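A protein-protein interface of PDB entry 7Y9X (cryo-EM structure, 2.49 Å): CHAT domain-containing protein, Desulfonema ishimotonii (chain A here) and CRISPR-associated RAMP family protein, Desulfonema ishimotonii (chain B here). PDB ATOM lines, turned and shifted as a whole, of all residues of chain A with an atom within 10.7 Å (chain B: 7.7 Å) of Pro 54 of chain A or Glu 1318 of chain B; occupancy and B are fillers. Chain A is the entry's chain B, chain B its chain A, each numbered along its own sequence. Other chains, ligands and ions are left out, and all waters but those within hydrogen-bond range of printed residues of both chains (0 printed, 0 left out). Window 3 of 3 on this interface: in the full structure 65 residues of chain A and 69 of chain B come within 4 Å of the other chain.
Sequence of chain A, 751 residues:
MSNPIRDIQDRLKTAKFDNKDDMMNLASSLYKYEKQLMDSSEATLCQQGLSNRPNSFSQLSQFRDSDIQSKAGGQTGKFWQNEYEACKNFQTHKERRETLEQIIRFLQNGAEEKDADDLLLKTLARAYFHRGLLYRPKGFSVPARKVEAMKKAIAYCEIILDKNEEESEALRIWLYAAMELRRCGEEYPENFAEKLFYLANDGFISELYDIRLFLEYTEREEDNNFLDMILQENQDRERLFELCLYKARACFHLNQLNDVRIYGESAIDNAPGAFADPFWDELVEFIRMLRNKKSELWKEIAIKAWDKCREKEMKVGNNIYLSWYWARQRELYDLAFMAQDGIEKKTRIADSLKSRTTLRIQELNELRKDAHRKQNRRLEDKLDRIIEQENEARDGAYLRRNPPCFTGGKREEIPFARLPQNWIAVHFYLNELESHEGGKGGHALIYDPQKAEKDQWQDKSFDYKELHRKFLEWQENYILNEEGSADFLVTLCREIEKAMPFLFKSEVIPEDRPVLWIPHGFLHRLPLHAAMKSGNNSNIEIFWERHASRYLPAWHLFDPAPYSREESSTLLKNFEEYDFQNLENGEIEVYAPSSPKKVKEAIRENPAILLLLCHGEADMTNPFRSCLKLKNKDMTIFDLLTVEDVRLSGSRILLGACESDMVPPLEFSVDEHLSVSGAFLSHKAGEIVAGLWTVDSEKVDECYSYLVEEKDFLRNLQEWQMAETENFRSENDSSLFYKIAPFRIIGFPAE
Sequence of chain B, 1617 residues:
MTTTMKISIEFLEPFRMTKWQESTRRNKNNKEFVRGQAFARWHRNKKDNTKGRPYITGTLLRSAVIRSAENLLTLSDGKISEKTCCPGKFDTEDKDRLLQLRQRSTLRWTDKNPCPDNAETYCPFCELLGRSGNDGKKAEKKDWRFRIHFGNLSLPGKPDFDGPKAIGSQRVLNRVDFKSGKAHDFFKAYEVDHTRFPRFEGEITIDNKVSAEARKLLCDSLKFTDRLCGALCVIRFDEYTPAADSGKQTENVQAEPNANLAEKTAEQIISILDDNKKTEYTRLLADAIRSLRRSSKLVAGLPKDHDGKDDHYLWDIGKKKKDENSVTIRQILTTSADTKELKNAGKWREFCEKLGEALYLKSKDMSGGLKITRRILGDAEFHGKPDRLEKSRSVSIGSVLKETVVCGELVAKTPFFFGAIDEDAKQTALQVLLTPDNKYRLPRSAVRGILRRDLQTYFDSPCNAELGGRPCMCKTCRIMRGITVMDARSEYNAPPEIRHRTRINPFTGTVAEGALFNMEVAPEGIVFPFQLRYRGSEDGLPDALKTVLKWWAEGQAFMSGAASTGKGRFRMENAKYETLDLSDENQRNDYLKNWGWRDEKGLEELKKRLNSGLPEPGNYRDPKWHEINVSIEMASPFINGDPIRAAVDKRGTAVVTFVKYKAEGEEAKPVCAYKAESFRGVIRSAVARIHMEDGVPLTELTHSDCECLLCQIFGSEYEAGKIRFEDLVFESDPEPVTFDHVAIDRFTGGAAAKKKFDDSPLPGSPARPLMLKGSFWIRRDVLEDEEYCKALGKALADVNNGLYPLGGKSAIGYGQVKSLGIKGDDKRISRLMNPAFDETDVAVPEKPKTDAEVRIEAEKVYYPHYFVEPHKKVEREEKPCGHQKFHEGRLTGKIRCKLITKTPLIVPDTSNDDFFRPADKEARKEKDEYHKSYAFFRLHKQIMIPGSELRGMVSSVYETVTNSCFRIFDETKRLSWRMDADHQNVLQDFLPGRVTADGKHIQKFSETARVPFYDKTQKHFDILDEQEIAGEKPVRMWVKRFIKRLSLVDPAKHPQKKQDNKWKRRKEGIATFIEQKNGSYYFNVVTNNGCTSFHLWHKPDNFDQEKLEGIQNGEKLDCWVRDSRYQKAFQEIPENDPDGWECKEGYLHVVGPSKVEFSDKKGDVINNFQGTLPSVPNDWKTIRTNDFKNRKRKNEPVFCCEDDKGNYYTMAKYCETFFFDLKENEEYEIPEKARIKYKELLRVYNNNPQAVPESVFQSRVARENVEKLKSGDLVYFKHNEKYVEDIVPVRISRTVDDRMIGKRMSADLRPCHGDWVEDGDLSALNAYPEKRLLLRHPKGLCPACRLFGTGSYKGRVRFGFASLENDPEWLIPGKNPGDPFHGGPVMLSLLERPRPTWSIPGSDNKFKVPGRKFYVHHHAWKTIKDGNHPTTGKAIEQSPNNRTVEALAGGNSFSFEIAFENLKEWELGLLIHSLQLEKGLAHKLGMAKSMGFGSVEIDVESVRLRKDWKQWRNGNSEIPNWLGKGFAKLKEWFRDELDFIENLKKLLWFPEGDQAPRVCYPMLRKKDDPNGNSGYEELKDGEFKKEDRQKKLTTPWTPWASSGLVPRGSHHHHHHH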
ATOM      1  N   GLN A   9      39.360  -3.853 -16.059  1.00  0.00           N
ATOM      2  CA  GLN A   9      39.608  -4.271 -17.434  1.00  0.00           C
ATOM      3  C   GLN A   9      41.021  -4.817 -17.600  1.00  0.00           C
ATOM      4  O   GLN A   9      41.237  -5.786 -18.335  1.00  0.00           O
ATOM      5  CB  GLN A   9      39.359  -3.099 -18.385  1.00  0.00           C
ATOM      6  CG  GLN A   9      39.552  -3.419 -19.857  1.00  0.00           C
ATOM      7  CD  GLN A   9      38.493  -4.355 -20.405  1.00  0.00           C
ATOM      8  OE1 GLN A   9      37.449  -4.560 -19.793  1.00  0.00           O
ATOM      9  NE2 GLN A   9      38.759  -4.926 -21.569  1.00  0.00           N
ATOM     10  N   LEU A  12      41.247  -8.267 -16.192  1.00  0.00           N
ATOM     11  CA  LEU A  12      40.594  -9.266 -17.029  1.00  0.00           C
ATOM     12  C   LEU A  12      41.477  -9.706 -18.189  1.00  0.00           C
ATOM     13  O   LEU A  12      41.342 -10.838 -18.668  1.00  0.00           O
ATOM     14  CB  LEU A  12      39.263  -8.721 -17.547  1.00  0.00           C
ATOM     15  CG  LEU A  12      38.155  -8.498 -16.516  1.00  0.00           C
ATOM     16  CD1 LEU A  12      36.940  -7.855 -17.164  1.00  0.00           C
ATOM     17  CD2 LEU A  12      37.771  -9.807 -15.849  1.00  0.00           C
ATOM     18  N   PHE A  17      42.514 -18.322 -13.657  1.00  0.00           N
ATOM     19  CA  PHE A  17      41.586 -18.614 -12.571  1.00  0.00           C
ATOM     20  C   PHE A  17      42.112 -19.697 -11.638  1.00  0.00           C
ATOM     21  O   PHE A  17      41.735 -19.728 -10.462  1.00  0.00           O
ATOM     22  CB  PHE A  17      40.222 -18.993 -13.143  1.00  0.00           C
ATOM     23  CG  PHE A  17      39.457 -17.818 -13.682  1.00  0.00           C
ATOM     24  CD1 PHE A  17      39.840 -17.211 -14.870  1.00  0.00           C
ATOM     25  CD2 PHE A  17      38.380 -17.298 -12.989  1.00  0.00           C
ATOM     26  CE1 PHE A  17      39.153 -16.123 -15.359  1.00  0.00           C
ATOM     27  CE2 PHE A  17      37.691 -16.209 -13.478  1.00  0.00           C
ATOM     28  CZ  PHE A  17      38.079 -15.622 -14.662  1.00  0.00           C
ATOM     29  N   LEU A  50      32.944  -1.981 -19.757  1.00  0.00           N
ATOM     30  CA  LEU A  50      34.021  -2.904 -20.082  1.00  0.00           C
ATOM     31  C   LEU A  50      34.035  -3.217 -21.572  1.00  0.00           C
ATOM     32  O   LEU A  50      32.987  -3.449 -22.179  1.00  0.00           O
ATOM     33  CB  LEU A  50      33.867  -4.201 -19.289  1.00  0.00           C
ATOM     34  CG  LEU A  50      33.995  -4.093 -17.774  1.00  0.00           C
ATOM     35  CD1 LEU A  50      33.646  -5.413 -17.125  1.00  0.00           C
ATOM     36  CD2 LEU A  50      35.393  -3.661 -17.389  1.00  0.00           C
ATOM     37  N   SER A  51      35.231  -3.232 -22.154  1.00  0.00           N
ATOM     38  CA  SER A  51      35.384  -3.616 -23.548  1.00  0.00           C
ATOM     39  C   SER A  51      35.417  -5.134 -23.682  1.00  0.00           C
ATOM     40  O   SER A  51      35.621  -5.864 -22.710  1.00  0.00           O
ATOM     41  CB  SER A  51      36.652  -3.007 -24.141  1.00  0.00           C
ATOM     42  OG  SER A  51      37.802  -3.445 -23.447  1.00  0.00           O
ATOM     43  N   ASN A  52      35.205  -5.604 -24.913  1.00  0.00           N
ATOM     44  CA  ASN A  52      35.174  -7.031 -25.240  1.00  0.00           C
ATOM     45  C   ASN A  52      34.136  -7.758 -24.380  1.00  0.00           C
ATOM     46  O   ASN A  52      34.453  -8.590 -23.531  1.00  0.00           O
ATOM     47  CB  ASN A  52      36.566  -7.656 -25.091  1.00  0.00           C
ATOM     48  CG  ASN A  52      36.662  -9.027 -25.727  1.00  0.00           C
ATOM     49  OD1 ASN A  52      35.714  -9.504 -26.350  1.00  0.00           O
ATOM     50  ND2 ASN A  52      37.816  -9.666 -25.583  1.00  0.00           N
ATOM     51  N   ARG A  53      32.876  -7.402 -24.627  1.00  0.00           N
ATOM     52  CA  ARG A  53      31.785  -7.867 -23.772  1.00  0.00           C
ATOM     53  C   ARG A  53      31.650  -9.384 -23.708  1.00  0.00           C
ATOM     54  O   ARG A  53      31.475  -9.910 -22.596  1.00  0.00           O
ATOM     55  CB  ARG A  53      30.471  -7.212 -24.212  1.00  0.00           C
ATOM     56  CG  ARG A  53      30.529  -5.707 -24.229  1.00  0.00           C
ATOM     57  CD  ARG A  53      29.200  -5.093 -24.595  1.00  0.00           C
ATOM     58  NE  ARG A  53      29.308  -3.645 -24.700  1.00  0.00           N
ATOM     59  CZ  ARG A  53      28.294  -2.832 -24.953  1.00  0.00           C
ATOM     60  NH1 ARG A  53      27.065  -3.291 -25.106  1.00  0.00           N
ATOM     61  NH2 ARG A  53      28.519  -1.527 -25.057  1.00  0.00           N
ATOM     62  N   PRO A  54      31.678 -10.137 -24.817  1.00  0.00           N
ATOM     63  CA  PRO A  54      31.551 -11.599 -24.682  1.00  0.00           C
ATOM     64  C   PRO A  54      32.646 -12.227 -23.838  1.00  0.00           C
ATOM     65  O   PRO A  54      32.369 -13.134 -23.043  1.00  0.00           O
ATOM     66  CB  PRO A  54      31.606 -12.086 -26.136  1.00  0.00           C
ATOM     67  CG  PRO A  54      31.171 -10.930 -26.937  1.00  0.00           C
ATOM     68  CD  PRO A  54      31.719  -9.734 -26.233  1.00  0.00           C
ATOM     69  N   ASN A  55      33.885 -11.758 -23.979  1.00  0.00           N
ATOM     70  CA  ASN A  55      34.981 -12.300 -23.183  1.00  0.00           C
ATOM     71  C   ASN A  55      34.950 -11.770 -21.755  1.00  0.00           C
ATOM     72  O   ASN A  55      35.231 -12.514 -20.810  1.00  0.00           O
ATOM     73  CB  ASN A  55      36.316 -11.973 -23.848  1.00  0.00           C
ATOM     74  CG  ASN A  55      37.490 -12.618 -23.148  1.00  0.00           C
ATOM     75  OD1 ASN A  55      37.348 -13.647 -22.494  1.00  0.00           O
ATOM     76  ND2 ASN A  55      38.662 -12.011 -23.285  1.00  0.00           N
ATOM     77  N   SER A  56      34.608 -10.492 -21.579  1.00  0.00           N
ATOM     78  CA  SER A  56      34.496  -9.935 -20.236  1.00  0.00           C
ATOM     79  C   SER A  56      33.383 -10.614 -19.451  1.00  0.00           C
ATOM     80  O   SER A  56      33.516 -10.844 -18.245  1.00  0.00           O
ATOM     81  CB  SER A  56      34.260  -8.427 -20.305  1.00  0.00           C
ATOM     82  OG  SER A  56      35.332  -7.769 -20.948  1.00  0.00           O
ATOM     83  N   PHE A  57      32.270 -10.927 -20.118  1.00  0.00           N
ATOM     84  CA  PHE A  57      31.168 -11.602 -19.444  1.00  0.00           C
ATOM     85  C   PHE A  57      31.557 -13.007 -19.000  1.00  0.00           C
ATOM     86  O   PHE A  57      31.180 -13.443 -17.906  1.00  0.00           O
ATOM     87  CB  PHE A  57      29.944 -11.651 -20.359  1.00  0.00           C
ATOM     88  CG  PHE A  57      28.876 -12.598 -19.891  1.00  0.00           C
ATOM     89  CD1 PHE A  57      28.098 -12.294 -18.792  1.00  0.00           C
ATOM     90  CD2 PHE A  57      28.650 -13.790 -20.554  1.00  0.00           C
ATOM     91  CE1 PHE A  57      27.119 -13.162 -18.360  1.00  0.00           C
ATOM     92  CE2 PHE A  57      27.674 -14.658 -20.126  1.00  0.00           C
ATOM     93  CZ  PHE A  57      26.908 -14.344 -19.028  1.00  0.00           C
ATOM     94  N   SER A  58      32.294 -13.739 -19.841  1.00  0.00           N
ATOM     95  CA  SER A  58      32.675 -15.104 -19.489  1.00  0.00           C
ATOM     96  C   SER A  58      33.651 -15.118 -18.319  1.00  0.00           C
ATOM     97  O   SER A  58      33.503 -15.913 -17.386  1.00  0.00           O
ATOM     98  CB  SER A  58      33.274 -15.816 -20.700  1.00  0.00           C
ATOM     99  OG  SER A  58      34.493 -15.219 -21.095  1.00  0.00           O
ATOM    100  N   GLN A  59      34.653 -14.236 -18.350  1.00  0.00           N
ATOM    101  CA  GLN A  59      35.614 -14.167 -17.255  1.00  0.00           C
ATOM    102  C   GLN A  59      34.935 -13.779 -15.950  1.00  0.00           C
ATOM    103  O   GLN A  59      35.232 -14.347 -14.894  1.00  0.00           O
ATOM    104  CB  GLN A  59      36.720 -13.173 -17.593  1.00  0.00           C
ATOM    105  CG  GLN A  59      37.564 -13.568 -18.784  1.00  0.00           C
ATOM    106  CD  GLN A  59      38.814 -12.726 -18.907  1.00  0.00           C
ATOM    107  OE1 GLN A  59      39.352 -12.547 -19.998  1.00  0.00           O
ATOM    108  NE2 GLN A  59      39.294 -12.216 -17.781  1.00  0.00           N
ATOM    109  N   LEU A  60      34.025 -12.808 -16.002  1.00  0.00           N
ATOM    110  CA  LEU A  60      33.321 -12.391 -14.795  1.00  0.00           C
ATOM    111  C   LEU A  60      32.402 -13.494 -14.288  1.00  0.00           C
ATOM    112  O   LEU A  60      32.234 -13.664 -13.076  1.00  0.00           O
ATOM    113  CB  LEU A  60      32.534 -11.110 -15.070  1.00  0.00           C
ATOM    114  CG  LEU A  60      33.370  -9.829 -15.113  1.00  0.00           C
ATOM    115  CD1 LEU A  60      32.547  -8.656 -15.618  1.00  0.00           C
ATOM    116  CD2 LEU A  60      33.973  -9.523 -13.749  1.00  0.00           C
ATOM    117  N   SER A  61      31.799 -14.256 -15.202  1.00  0.00           N
ATOM    118  CA  SER A  61      30.921 -15.344 -14.795  1.00  0.00           C
ATOM    119  C   SER A  61      31.701 -16.487 -14.153  1.00  0.00           C
ATOM    120  O   SER A  61      31.221 -17.093 -13.189  1.00  0.00           O
ATOM    121  CB  SER A  61      30.119 -15.844 -15.996  1.00  0.00           C
ATOM    122  OG  SER A  61      28.954 -16.534 -15.584  1.00  0.00           O
ATOM    123  N   GLN A  62      32.891 -16.802 -14.674  1.00  0.00           N
ATOM    124  CA  GLN A  62      33.720 -17.835 -14.057  1.00  0.00           C
ATOM    125  C   GLN A  62      34.198 -17.414 -12.674  1.00  0.00           C
ATOM    126  O   GLN A  62      34.254 -18.235 -11.751  1.00  0.00           O
ATOM    127  CB  GLN A  62      34.917 -18.164 -14.948  1.00  0.00           C
ATOM    128  CG  GLN A  62      34.549 -18.666 -16.329  1.00  0.00           C
ATOM    129  CD  GLN A  62      35.759 -18.863 -17.213  1.00  0.00           C
ATOM    130  OE1 GLN A  62      36.895 -18.811 -16.747  1.00  0.00           O
ATOM    131  NE2 GLN A  62      35.520 -19.088 -18.498  1.00  0.00           N
ATOM    132  N   THR B 972      16.858  -5.520 -28.609  1.00  0.00           N
ATOM    133  CA  THR B 972      16.608  -6.952 -28.518  1.00  0.00           C
ATOM    134  C   THR B 972      15.559  -7.435 -29.508  1.00  0.00           C
ATOM    135  O   THR B 972      15.219  -8.623 -29.490  1.00  0.00           O
ATOM    136  CB  THR B 972      16.192  -7.320 -27.093  1.00  0.00           C
ATOM    137  OG1 THR B 972      15.047  -6.552 -26.710  1.00  0.00           O
ATOM    138  CG2 THR B 972      17.320  -7.031 -26.125  1.00  0.00           C
ATOM    139  N   ARG B 974      14.062  -8.938 -32.772  1.00  0.00           N
ATOM    140  CA  ARG B 974      14.546  -9.914 -33.737  1.00  0.00           C
ATOM    141  C   ARG B 974      13.643  -9.875 -34.963  1.00  0.00           C
ATOM    142  O   ARG B 974      12.435 -10.102 -34.853  1.00  0.00           O
ATOM    143  CB  ARG B 974      14.573 -11.308 -33.112  1.00  0.00           C
ATOM    144  CG  ARG B 974      15.252 -12.363 -33.949  1.00  0.00           C
ATOM    145  CD  ARG B 974      15.236 -13.701 -33.235  1.00  0.00           C
ATOM    146  NE  ARG B 974      15.963 -13.670 -31.971  1.00  0.00           N
ATOM    147  CZ  ARG B 974      17.237 -14.008 -31.834  1.00  0.00           C
ATOM    148  NH1 ARG B 974      17.962 -14.403 -32.866  1.00  0.00           N
ATOM    149  NH2 ARG B 974      17.797 -13.950 -30.629  1.00  0.00           N
ATOM    150  N   MET B1300      19.701 -10.355 -33.107  1.00  0.00           N
ATOM    151  CA  MET B1300      18.907  -9.208 -32.709  1.00  0.00           C
ATOM    152  C   MET B1300      19.235  -8.025 -33.614  1.00  0.00           C
ATOM    153  O   MET B1300      20.315  -7.944 -34.205  1.00  0.00           O
ATOM    154  CB  MET B1300      19.178  -8.850 -31.253  1.00  0.00           C
ATOM    155  CG  MET B1300      18.787  -9.925 -30.270  1.00  0.00           C
ATOM    156  SD  MET B1300      19.159  -9.445 -28.579  1.00  0.00           S
ATOM    157  CE  MET B1300      18.560 -10.868 -27.687  1.00  0.00           C
ATOM    158  N   LYS B1303      22.576  -5.987 -33.383  1.00  0.00           N
ATOM    159  CA  LYS B1303      23.773  -6.372 -34.117  1.00  0.00           C
ATOM    160  C   LYS B1303      23.769  -5.890 -35.559  1.00  0.00           C
ATOM    161  O   LYS B1303      24.799  -5.995 -36.230  1.00  0.00           O
ATOM    162  CB  LYS B1303      23.942  -7.887 -34.089  1.00  0.00           C
ATOM    163  CG  LYS B1303      24.496  -8.429 -32.789  1.00  0.00           C
ATOM    164  CD  LYS B1303      25.858  -7.827 -32.491  1.00  0.00           C
ATOM    165  CE  LYS B1303      26.665  -8.719 -31.566  1.00  0.00           C
ATOM    166  NZ  LYS B1303      25.885  -9.128 -30.374  1.00  0.00           N
ATOM    167  N   ALA B1307      28.200  -0.794 -33.363  1.00  0.00           N
ATOM    168  CA  ALA B1307      28.217  -0.839 -31.906  1.00  0.00           C
ATOM    169  C   ALA B1307      28.377   0.550 -31.303  1.00  0.00           C
ATOM    170  O   ALA B1307      27.956   0.785 -30.166  1.00  0.00           O
ATOM    171  CB  ALA B1307      29.329  -1.767 -31.424  1.00  0.00           C
ATOM    172  N   ARG B1310      24.796   2.169 -31.108  1.00  0.00           N
ATOM    173  CA  ARG B1310      23.873   1.649 -30.125  1.00  0.00           C
ATOM    174  C   ARG B1310      23.836   2.573 -28.912  1.00  0.00           C
ATOM    175  O   ARG B1310      24.777   3.331 -28.675  1.00  0.00           O
ATOM    176  CB  ARG B1310      24.285   0.241 -29.714  1.00  0.00           C
ATOM    177  CG  ARG B1310      24.152  -0.791 -30.811  1.00  0.00           C
ATOM    178  CD  ARG B1310      24.751  -2.099 -30.372  1.00  0.00           C
ATOM    179  NE  ARG B1310      24.156  -2.583 -29.135  1.00  0.00           N
ATOM    180  CZ  ARG B1310      24.623  -3.607 -28.436  1.00  0.00           C
ATOM    181  NH1 ARG B1310      25.703  -4.266 -28.817  1.00  0.00           N
ATOM    182  NH2 ARG B1310      23.995  -3.971 -27.321  1.00  0.00           N
ATOM    183  N   ASP B1315      20.910  -2.492 -23.798  1.00  0.00           N
ATOM    184  CA  ASP B1315      20.608  -3.875 -23.457  1.00  0.00           C
ATOM    185  C   ASP B1315      21.677  -4.814 -24.000  1.00  0.00           C
ATOM    186  O   ASP B1315      22.552  -4.427 -24.777  1.00  0.00           O
ATOM    187  CB  ASP B1315      19.228  -4.286 -23.987  1.00  0.00           C
ATOM    188  CG  ASP B1315      18.094  -3.541 -23.316  1.00  0.00           C
ATOM    189  OD1 ASP B1315      18.224  -3.194 -22.126  1.00  0.00           O
ATOM    190  OD2 ASP B1315      17.064  -3.310 -23.978  1.00  0.00           O
ATOM    191  N   TRP B1316      21.578  -6.071 -23.574  1.00  0.00           N
ATOM    192  CA  TRP B1316      22.537  -7.115 -23.909  1.00  0.00           C
ATOM    193  C   TRP B1316      22.052  -7.891 -25.127  1.00  0.00           C
ATOM    194  O   TRP B1316      21.018  -8.562 -25.069  1.00  0.00           O
ATOM    195  CB  TRP B1316      22.729  -8.036 -22.706  1.00  0.00           C
ATOM    196  CG  TRP B1316      23.733  -9.137 -22.870  1.00  0.00           C
ATOM    197  CD1 TRP B1316      23.470 -10.445 -23.151  1.00  0.00           C
ATOM    198  CD2 TRP B1316      25.156  -9.028 -22.766  1.00  0.00           C
ATOM    199  NE1 TRP B1316      24.637 -11.159 -23.218  1.00  0.00           N
ATOM    200  CE2 TRP B1316      25.688 -10.313 -22.985  1.00  0.00           C
ATOM    201  CE3 TRP B1316      26.032  -7.972 -22.505  1.00  0.00           C
ATOM    202  CZ2 TRP B1316      27.056 -10.568 -22.952  1.00  0.00           C
ATOM    203  CZ3 TRP B1316      27.385  -8.227 -22.474  1.00  0.00           C
ATOM    204  CH2 TRP B1316      27.886  -9.513 -22.698  1.00  0.00           C
ATOM    205  N   VAL B1317      22.800  -7.795 -26.226  1.00  0.00           N
ATOM    206  CA  VAL B1317      22.462  -8.472 -27.472  1.00  0.00           C
ATOM    207  C   VAL B1317      23.402  -9.624 -27.781  1.00  0.00           C
ATOM    208  O   VAL B1317      23.363 -10.157 -28.898  1.00  0.00           O
ATOM    209  CB  VAL B1317      22.426  -7.486 -28.656  1.00  0.00           C
ATOM    210  CG1 VAL B1317      21.459  -6.348 -28.376  1.00  0.00           C
ATOM    211  CG2 VAL B1317      23.811  -6.962 -28.954  1.00  0.00           C
ATOM    212  N   GLU B1318      24.246 -10.024 -26.836  1.00  0.00           N
ATOM    213  CA  GLU B1318      25.174 -11.118 -27.061  1.00  0.00           C
ATOM    214  C   GLU B1318      24.541 -12.447 -26.656  1.00  0.00           C
ATOM    215  O   GLU B1318      23.415 -12.508 -26.157  1.00  0.00           O
ATOM    216  CB  GLU B1318      26.467 -10.893 -26.283  1.00  0.00           C
ATOM    217  CG  GLU B1318      27.016  -9.479 -26.348  1.00  0.00           C
ATOM    218  CD  GLU B1318      27.611  -9.132 -27.692  1.00  0.00           C
ATOM    219  OE1 GLU B1318      27.907 -10.058 -28.476  1.00  0.00           O
ATOM    220  OE2 GLU B1318      27.785  -7.927 -27.965  1.00  0.00           O
ATOM    221  N   ASP B1319      25.281 -13.527 -26.889  1.00  0.00           N
ATOM    222  CA  ASP B1319      24.820 -14.850 -26.491  1.00  0.00           C
ATOM    223  C   ASP B1319      24.976 -15.039 -24.987  1.00  0.00           C
ATOM    224  O   ASP B1319      25.901 -14.509 -24.367  1.00  0.00           O
ATOM    225  CB  ASP B1319      25.590 -15.932 -27.243  1.00  0.00           C
ATOM    226  CG  ASP B1319      25.296 -15.926 -28.728  1.00  0.00           C
ATOM    227  OD1 ASP B1319      24.174 -15.536 -29.111  1.00  0.00           O
ATOM    228  OD2 ASP B1319      26.187 -16.312 -29.513  1.00  0.00           O
ATOM    229  N   GLY B1320      24.066 -15.810 -24.403  1.00  0.00           N
ATOM    230  CA  GLY B1320      24.025 -15.979 -22.968  1.00  0.00           C
ATOM    231  C   GLY B1320      23.201 -14.897 -22.299  1.00  0.00           C
ATOM    232  O   GLY B1320      22.807 -13.898 -22.903  1.00  0.00           O
ATOM    233  N   ASP B1321      22.934 -15.106 -21.015  1.00  0.00           N
ATOM    234  CA  ASP B1321      22.110 -14.192 -20.241  1.00  0.00           C
ATOM    235  C   ASP B1321      22.946 -13.513 -19.166  1.00  0.00           C
ATOM    236  O   ASP B1321      23.711 -14.169 -18.453  1.00  0.00           O
ATOM    237  CB  ASP B1321      20.922 -14.922 -19.604  1.00  0.00           C
ATOM    238  CG  ASP B1321      21.350 -16.073 -18.716  1.00  0.00           C
ATOM    239  OD1 ASP B1321      22.374 -16.716 -19.025  1.00  0.00           O
ATOM    240  OD2 ASP B1321      20.659 -16.335 -17.710  1.00  0.00           O
ATOM    241  N   LEU B1322      22.803 -12.191 -19.064  1.00  0.00           N
ATOM    242  CA  LEU B1322      23.428 -11.435 -17.987  1.00  0.00           C
ATOM    243  C   LEU B1322      22.798 -11.706 -16.630  1.00  0.00           C
ATOM    244  O   LEU B1322      23.352 -11.272 -15.617  1.00  0.00           O
ATOM    245  CB  LEU B1322      23.358  -9.934 -18.269  1.00  0.00           C
ATOM    246  CG  LEU B1322      24.248  -9.345 -19.356  1.00  0.00           C
ATOM    247  CD1 LEU B1322      24.161  -7.840 -19.301  1.00  0.00           C
ATOM    248  CD2 LEU B1322      25.681  -9.797 -19.173  1.00  0.00           C
ATOM    249  N   LEU B1334      28.877  -4.267 -18.256  1.00  0.00           N
ATOM    250  CA  LEU B1334      28.652  -4.996 -19.493  1.00  0.00           C
ATOM    251  C   LEU B1334      27.531  -4.395 -20.328  1.00  0.00           C
ATOM    252  O   LEU B1334      27.293  -4.860 -21.446  1.00  0.00           O
ATOM    253  CB  LEU B1334      28.348  -6.462 -19.182  1.00  0.00           C
ATOM    254  CG  LEU B1334      29.478  -7.253 -18.520  1.00  0.00           C
ATOM    255  CD1 LEU B1334      29.006  -8.634 -18.143  1.00  0.00           C
ATOM    256  CD2 LEU B1334      30.662  -7.344 -19.456  1.00  0.00           C
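O of Ser 51 of chain A lies within hydrogen-bond range of OG of Ser 56 of chain A, at 2.6 Å. OG of Ser 56 of chain A is in hydrogen-bond range of O of Asn 52 of chain A, 2.8 Å away. NZ of Lys 1303 of chain B is in salt-bridge range of OE1 of Glu 1318 of chain B (2.9 Å). The guanidinium group (NH2) of Arg 1310 of chain B lies within hydrogen-bond range of the backbone carbonyl oxygen (O) of Asp 1315 of chain B (3.0 Å). The backbone carbonyl oxygen (O) of Glu 1318 of chain B sits at hydrogen-bond distance from the indole nitrogen (NE1) of Trp 1316 of chain B (3.5 Å). O of Gly 1320 of chain B is in hydrogen-bond range of NE1 of Trp 1316 of chain B, at 3.3 Å.
Arg 53 of chain A touches Arg 1310 of chain B. Arg 53 of chain A touches Trp 1316 of chain B (O to CH2, 3.6 Å). Leu 1334 of chain B touches Arg 53 of chain A. Pro 54 of chain A touches Glu 1318 of chain B. CB of Ser 56 of chain A touches CD2 of Leu 1334 of chain B, at 3.9 Å. CB of Phe 57 of chain A touches CH2 of Trp 1316 of chain B, 3.8 Å away. Asp 1321 of chain B touches Phe 57 of chain A. CD1 of Phe 57 of chain A touches CD2 of Leu 1322 of chain B (3.5 Å). Phe 57 of chain A touches Leu 1334 of chain B.
Of chain B, only Glu 1318 (3.7 Å) comes within 4 Å of Pro 54 of chain A. Glu 1318 of chain B touches just one residue of chain A: Pro 54. Trp 1316 of chain B touches just these residues of chain A: Arg 53 and Phe 57. No residue of chain A comes within 4 Å of Val 1317 of chain B. No residue of chain A comes within 4 Å of Asp 1319 of chain B. No residue of chain A comes within 4 Å of Gly 1320 of chain B. Of the printed residues of chain B, Phe 57 of chain A touches Trp 1316, Asp 1321, Leu 1322 and Leu 1334. Of the printed residues of chain B, Ser 56 of chain A touches Leu 1334. Of the printed residues of chain A, Leu 1322 of chain B touches Phe 57 (3.5 Å). The nearest residue of chain B that does not touch Pro 54 of chain A is Trp 1316 of chain B (4.4 Å).
Hydrophobic or aromatic side chains of chain A that line the printed part of chain B: Pro 54 and Phe 57. Hydrophobic or aromatic side chains of chain B that line the printed part of chain A: Trp 1316, Leu 1322 and Leu 1334. Among the printed residues, no Asp or Glu carboxylate lies within 4 Å of a Lys or Arg side-chain nitrogen of the other chain.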
